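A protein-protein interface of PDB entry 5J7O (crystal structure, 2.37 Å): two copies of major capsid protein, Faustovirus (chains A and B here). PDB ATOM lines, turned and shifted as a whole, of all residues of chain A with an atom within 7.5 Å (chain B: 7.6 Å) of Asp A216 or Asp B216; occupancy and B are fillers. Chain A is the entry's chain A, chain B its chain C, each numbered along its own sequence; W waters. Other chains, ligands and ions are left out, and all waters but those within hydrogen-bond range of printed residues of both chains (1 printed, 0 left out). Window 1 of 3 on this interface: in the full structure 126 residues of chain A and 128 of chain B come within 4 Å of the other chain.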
ATOM      1  N   VAL A 214      13.065  18.097  -2.507  1.00  0.00           N
ATOM      2  CA  VAL A 214      11.903  17.994  -3.389  1.00  0.00           C
ATOM      3  C   VAL A 214      11.017  19.216  -3.181  1.00  0.00           C
ATOM      4  O   VAL A 214      10.130  19.203  -2.316  1.00  0.00           O
ATOM      5  CB  VAL A 214      11.120  16.691  -3.154  1.00  0.00           C
ATOM      6  CG1 VAL A 214       9.970  16.582  -4.146  1.00  0.00           C
ATOM      7  CG2 VAL A 214      12.041  15.488  -3.276  1.00  0.00           C
ATOM      8  N   PRO A 215      11.229  20.292  -3.934  1.00  0.00           N
ATOM      9  CA  PRO A 215      10.341  21.455  -3.835  1.00  0.00           C
ATOM     10  C   PRO A 215       8.959  21.138  -4.387  1.00  0.00           C
ATOM     11  O   PRO A 215       8.729  20.112  -5.031  1.00  0.00           O
ATOM     12  CB  PRO A 215      11.054  22.524  -4.668  1.00  0.00           C
ATOM     13  CG  PRO A 215      11.925  21.750  -5.601  1.00  0.00           C
ATOM     14  CD  PRO A 215      12.350  20.524  -4.860  1.00  0.00           C
ATOM     15  N   ASP A 216       8.025  22.055  -4.124  1.00  0.00           N
ATOM     16  CA  ASP A 216       6.625  21.804  -4.453  1.00  0.00           C
ATOM     17  C   ASP A 216       6.405  21.631  -5.951  1.00  0.00           C
ATOM     18  O   ASP A 216       5.504  20.886  -6.357  1.00  0.00           O
ATOM     19  CB  ASP A 216       5.745  22.933  -3.917  1.00  0.00           C
ATOM     20  CG  ASP A 216       5.427  22.774  -2.442  1.00  0.00           C
ATOM     21  OD1 ASP A 216       4.486  22.021  -2.114  1.00  0.00           O
ATOM     22  OD2 ASP A 216       6.116  23.403  -1.611  1.00  0.00           O
ATOM     23  N   PHE A 217       7.206  22.292  -6.790  1.00  0.00           N
ATOM     24  CA  PHE A 217       6.990  22.120  -8.223  1.00  0.00           C
ATOM     25  C   PHE A 217       7.467  20.765  -8.738  1.00  0.00           C
ATOM     26  O   PHE A 217       7.311  20.490  -9.932  1.00  0.00           O
ATOM     27  CB  PHE A 217       7.644  23.259  -9.018  1.00  0.00           C
ATOM     28  CG  PHE A 217       9.093  23.501  -8.692  1.00  0.00           C
ATOM     29  CD1 PHE A 217      10.091  22.755  -9.298  1.00  0.00           C
ATOM     30  CD2 PHE A 217       9.459  24.512  -7.818  1.00  0.00           C
ATOM     31  CE1 PHE A 217      11.424  22.992  -9.015  1.00  0.00           C
ATOM     32  CE2 PHE A 217      10.789  24.755  -7.532  1.00  0.00           C
ATOM     33  CZ  PHE A 217      11.772  23.996  -8.133  1.00  0.00           C
ATOM     34  N   LYS A 218       8.027  19.918  -7.873  1.00  0.00           N
ATOM     35  CA  LYS A 218       8.354  18.541  -8.215  1.00  0.00           C
ATOM     36  C   LYS A 218       7.674  17.529  -7.305  1.00  0.00           C
ATOM     37  O   LYS A 218       7.882  16.323  -7.483  1.00  0.00           O
ATOM     38  CB  LYS A 218       9.872  18.315  -8.154  1.00  0.00           C
ATOM     39  CG  LYS A 218      10.699  19.278  -8.982  1.00  0.00           C
ATOM     40  CD  LYS A 218      10.433  19.105 -10.465  1.00  0.00           C
ATOM     41  CE  LYS A 218      11.417  19.910 -11.293  1.00  0.00           C
ATOM     42  NZ  LYS A 218      11.172  19.754 -12.751  1.00  0.00           N
ATOM     43  N   LEU A 219       6.860  17.980  -6.347  1.00  0.00           N
ATOM     44  CA  LEU A 219       6.450  17.107  -5.251  1.00  0.00           C
ATOM     45  C   LEU A 219       5.458  16.040  -5.703  1.00  0.00           C
ATOM     46  O   LEU A 219       5.584  14.872  -5.321  1.00  0.00           O
ATOM     47  CB  LEU A 219       5.859  17.938  -4.112  1.00  0.00           C
ATOM     48  CG  LEU A 219       5.514  17.139  -2.855  1.00  0.00           C
ATOM     49  CD1 LEU A 219       6.698  16.283  -2.434  1.00  0.00           C
ATOM     50  CD2 LEU A 219       5.091  18.064  -1.724  1.00  0.00           C
ATOM     51  N   THR A 220       4.460  16.422  -6.504  1.00  0.00           N
ATOM     52  CA  THR A 220       3.413  15.474  -6.880  1.00  0.00           C
ATOM     53  C   THR A 220       3.983  14.294  -7.660  1.00  0.00           C
ATOM     54  O   THR A 220       3.597  13.142  -7.431  1.00  0.00           O
ATOM     55  CB  THR A 220       2.330  16.185  -7.691  1.00  0.00           C
ATOM     56  OG1 THR A 220       1.655  17.135  -6.856  1.00  0.00           O
ATOM     57  CG2 THR A 220       1.317  15.186  -8.234  1.00  0.00           C
ATOM     58  N   GLY A 221       4.917  14.559  -8.572  1.00  0.00           N
ATOM     59  CA  GLY A 221       5.485  13.484  -9.367  1.00  0.00           C
ATOM     60  C   GLY A 221       6.433  12.629  -8.559  1.00  0.00           C
ATOM     61  O   GLY A 221       6.425  11.401  -8.674  1.00  0.00           O
ATOM     62  N   VAL A 559      15.307  22.643   0.449  1.00  0.00           N
ATOM     63  CA  VAL A 559      13.960  22.865   0.960  1.00  0.00           C
ATOM     64  C   VAL A 559      14.004  22.848   2.481  1.00  0.00           C
ATOM     65  O   VAL A 559      14.626  21.961   3.081  1.00  0.00           O
ATOM     66  CB  VAL A 559      12.982  21.803   0.430  1.00  0.00           C
ATOM     67  CG1 VAL A 559      11.607  21.975   1.064  1.00  0.00           C
ATOM     68  CG2 VAL A 559      12.892  21.875  -1.086  1.00  0.00           C
ATOM     69  N   THR A 560      13.359  23.826   3.103  1.00  0.00           N
ATOM     70  CA  THR A 560      13.176  23.804   4.545  1.00  0.00           C
ATOM     71  C   THR A 560      12.337  22.586   4.918  1.00  0.00           C
ATOM     72  O   THR A 560      11.174  22.493   4.498  1.00  0.00           O
ATOM     73  CB  THR A 560      12.502  25.084   5.027  1.00  0.00           C
ATOM     74  OG1 THR A 560      11.311  25.318   4.264  1.00  0.00           O
ATOM     75  CG2 THR A 560      13.441  26.272   4.875  1.00  0.00           C
ATOM     76  N   GLN A 562       9.915  19.711   6.347  1.00  0.00           N
ATOM     77  CA  GLN A 562       8.707  19.634   7.160  1.00  0.00           C
ATOM     78  C   GLN A 562       8.970  18.879   8.457  1.00  0.00           C
ATOM     79  O   GLN A 562       8.444  19.246   9.515  1.00  0.00           O
ATOM     80  CB  GLN A 562       7.588  18.960   6.367  1.00  0.00           C
ATOM     81  CG  GLN A 562       6.189  19.269   6.867  1.00  0.00           C
ATOM     82  CD  GLN A 562       5.711  20.639   6.431  1.00  0.00           C
ATOM     83  OE1 GLN A 562       6.236  21.218   5.479  1.00  0.00           O
ATOM     84  NE2 GLN A 562       4.711  21.167   7.127  1.00  0.00           N
ATOM     85  N   HIS B 213       8.628  37.381  -1.240  1.00  0.00           N
ATOM     86  CA  HIS B 213       9.944  36.768  -1.385  1.00  0.00           C
ATOM     87  C   HIS B 213      10.117  35.493  -0.565  1.00  0.00           C
ATOM     88  O   HIS B 213      11.250  35.137  -0.226  1.00  0.00           O
ATOM     89  CB  HIS B 213      11.041  37.770  -1.018  1.00  0.00           C
ATOM     90  CG  HIS B 213      10.997  39.033  -1.819  1.00  0.00           C
ATOM     91  ND1 HIS B 213      11.045  39.042  -3.197  1.00  0.00           N
ATOM     92  CD2 HIS B 213      10.909  40.329  -1.438  1.00  0.00           C
ATOM     93  CE1 HIS B 213      10.987  40.288  -3.629  1.00  0.00           C
ATOM     94  NE2 HIS B 213      10.905  41.090  -2.581  1.00  0.00           N
ATOM     95  N   VAL B 214       9.036  34.790  -0.241  1.00  0.00           N
ATOM     96  CA  VAL B 214       9.164  33.505   0.448  1.00  0.00           C
ATOM     97  C   VAL B 214       8.386  32.448  -0.326  1.00  0.00           C
ATOM     98  O   VAL B 214       7.196  32.229  -0.054  1.00  0.00           O
ATOM     99  CB  VAL B 214       8.683  33.590   1.906  1.00  0.00           C
ATOM    100  CG1 VAL B 214       8.982  32.285   2.629  1.00  0.00           C
ATOM    101  CG2 VAL B 214       9.341  34.759   2.624  1.00  0.00           C
ATOM    102  N   PRO B 215       9.006  31.777  -1.293  1.00  0.00           N
ATOM    103  CA  PRO B 215       8.314  30.702  -2.014  1.00  0.00           C
ATOM    104  C   PRO B 215       8.097  29.489  -1.120  1.00  0.00           C
ATOM    105  O   PRO B 215       8.594  29.404   0.005  1.00  0.00           O
ATOM    106  CB  PRO B 215       9.256  30.386  -3.179  1.00  0.00           C
ATOM    107  CG  PRO B 215      10.597  30.848  -2.711  1.00  0.00           C
ATOM    108  CD  PRO B 215      10.350  32.036  -1.834  1.00  0.00           C
ATOM    109  N   ASP B 216       7.340  28.528  -1.654  1.00  0.00           N
ATOM    110  CA  ASP B 216       6.879  27.409  -0.838  1.00  0.00           C
ATOM    111  C   ASP B 216       8.018  26.498  -0.394  1.00  0.00           C
ATOM    112  O   ASP B 216       7.921  25.873   0.668  1.00  0.00           O
ATOM    113  CB  ASP B 216       5.821  26.606  -1.594  1.00  0.00           C
ATOM    114  CG  ASP B 216       4.433  27.203  -1.460  1.00  0.00           C
ATOM    115  OD1 ASP B 216       4.188  27.923  -0.470  1.00  0.00           O
ATOM    116  OD2 ASP B 216       3.583  26.947  -2.338  1.00  0.00           O
ATOM    117  N   PHE B 217       9.098  26.405  -1.170  1.00  0.00           N
ATOM    118  CA  PHE B 217      10.208  25.556  -0.747  1.00  0.00           C
ATOM    119  C   PHE B 217      11.043  26.183   0.364  1.00  0.00           C
ATOM    120  O   PHE B 217      12.006  25.558   0.820  1.00  0.00           O
ATOM    121  CB  PHE B 217      11.100  25.184  -1.941  1.00  0.00           C
ATOM    122  CG  PHE B 217      11.568  26.354  -2.761  1.00  0.00           C
ATOM    123  CD1 PHE B 217      12.704  27.062  -2.404  1.00  0.00           C
ATOM    124  CD2 PHE B 217      10.896  26.718  -3.918  1.00  0.00           C
ATOM    125  CE1 PHE B 217      13.145  28.126  -3.167  1.00  0.00           C
ATOM    126  CE2 PHE B 217      11.331  27.780  -4.685  1.00  0.00           C
ATOM    127  CZ  PHE B 217      12.459  28.482  -4.311  1.00  0.00           C
ATOM    128  N   LYS B 218      10.690  27.386   0.816  1.00  0.00           N
ATOM    129  CA  LYS B 218      11.315  28.010   1.973  1.00  0.00           C
ATOM    130  C   LYS B 218      10.312  28.374   3.060  1.00  0.00           C
ATOM    131  O   LYS B 218      10.716  28.909   4.099  1.00  0.00           O
ATOM    132  CB  LYS B 218      12.075  29.278   1.558  1.00  0.00           C
ATOM    133  CG  LYS B 218      13.127  29.070   0.487  1.00  0.00           C
ATOM    134  CD  LYS B 218      14.246  28.171   0.978  1.00  0.00           C
ATOM    135  CE  LYS B 218      15.460  28.274   0.073  1.00  0.00           C
ATOM    136  NZ  LYS B 218      16.588  27.427   0.554  1.00  0.00           N
ATOM    137  N   LEU B 219       9.024  28.090   2.857  1.00  0.00           N
ATOM    138  CA  LEU B 219       7.988  28.678   3.700  1.00  0.00           C
ATOM    139  C   LEU B 219       7.955  28.043   5.085  1.00  0.00           C
ATOM    140  O   LEU B 219       7.875  28.751   6.097  1.00  0.00           O
ATOM    141  CB  LEU B 219       6.627  28.552   3.018  1.00  0.00           C
ATOM    142  CG  LEU B 219       5.456  29.183   3.772  1.00  0.00           C
ATOM    143  CD1 LEU B 219       5.736  30.652   4.053  1.00  0.00           C
ATOM    144  CD2 LEU B 219       4.165  29.019   2.987  1.00  0.00           C
ATOM    145  N   THR B 220       7.995  26.710   5.152  1.00  0.00           N
ATOM    146  CA  THR B 220       7.882  26.031   6.441  1.00  0.00           C
ATOM    147  C   THR B 220       8.983  26.472   7.397  1.00  0.00           C
ATOM    148  O   THR B 220       8.719  26.755   8.571  1.00  0.00           O
ATOM    149  CB  THR B 220       7.912  24.515   6.242  1.00  0.00           C
ATOM    150  OG1 THR B 220       6.743  24.105   5.522  1.00  0.00           O
ATOM    151  CG2 THR B 220       7.940  23.802   7.583  1.00  0.00           C
ATOM    152  N   GLY B 221      10.223  26.551   6.912  1.00  0.00           N
ATOM    153  CA  GLY B 221      11.295  27.067   7.746  1.00  0.00           C
ATOM    154  C   GLY B 221      11.132  28.543   8.053  1.00  0.00           C
ATOM    155  O   GLY B 221      11.420  28.989   9.167  1.00  0.00           O
ATOM    156  N   VAL B 559       7.332  36.143  -5.634  1.00  0.00           N
ATOM    157  CA  VAL B 559       6.173  35.311  -5.337  1.00  0.00           C
ATOM    158  C   VAL B 559       4.912  36.128  -5.578  1.00  0.00           C
ATOM    159  O   VAL B 559       4.806  37.271  -5.116  1.00  0.00           O
ATOM    160  CB  VAL B 559       6.221  34.790  -3.890  1.00  0.00           C
ATOM    161  CG1 VAL B 559       4.933  34.061  -3.539  1.00  0.00           C
ATOM    162  CG2 VAL B 559       7.425  33.884  -3.691  1.00  0.00           C
HETATM  163  O   HOH W   1       8.422  24.543   2.784  1.00  0.00           O
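Phe B217 touches Pro A215.
Asp B216 touches Asp A216.
Val A559 touches Phe B217 (CA to O, 3.3 Å).
C of Lys B218 touches OG1 of Thr A560 (3.4 Å).
Leu B219 touches Thr A560 (N to OG1, 3.9 Å).
OG1 of Thr A560 touches N of Thr B220, at 3.7 Å.
Hydrophobic or aromatic side chains of chain B within 4 Å of the printed part of chain A: Phe B217.
Printed residues of chain A that touch a printed residue of chain B: Pro A215, Asp A216, Val A559, Thr A560 and Gln A562.
Hydrophobic or aromatic side chains of chain A within 4 Å of the printed part of chain B: Pro A215 and Val A559.
Among the printed residues, no Asp or Glu carboxylate lies within 4 Å of a Lys or Arg side-chain nitrogen of the other chain.
Pro A215 touches Phe B217, but with the chains exchanged Phe A217 does not touch Pro B215 (7.3 Å).
Asp B216 touches its own counterpart, Asp A216.
Val A559 touches Phe B217, but with the chains exchanged Phe A217 does not touch Val B559 (10.4 Å).
9 positions are printed for both chains.
OG1 of Thr A560 lies within hydrogen-bond range of N of Gly B221, at 3.1 Å.
N of Thr A560 lies within hydrogen-bond range of O of Phe B217 (3.2 Å).
The side-chain amide oxygen of Gln A562 lies within hydrogen-bond range of the side-chain hydroxyl of Thr B220 (2.9 Å).
Asp A216 touches just one residue of chain B: Asp B216.
Of chain A, only Asp A216 comes within 4 Å of Asp B216.
Of the printed residues of chain A, Thr B220 touches Thr A560 and Gln A562.
Of the printed residues of chain B, Pro A215 touches Phe B217 (3.8 Å).
Printed residues of chain B within 4 Å of Gln A562: Thr B220 (2.9 Å).
Printed residues of chain B within 4 Å of Val A559: Phe B217.
Pro B215 touches none of the printed residues of chain A.
The nearest residue of chain B that does not touch Asp A216 is Phe B217 (4.3 Å).
The nearest residue of chain A that does not touch Asp B216 is Thr A560 (5.0 Å).
The nearest printed residue of chain B that does not touch Thr A560 is Asp B216 (5.0 Å).
Water W1 lies within hydrogen-bond range of O of Asp B216 (2.5 Å), N of Thr B220 (3.2 Å) and OG1 of Thr A560 (3.3 Å).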
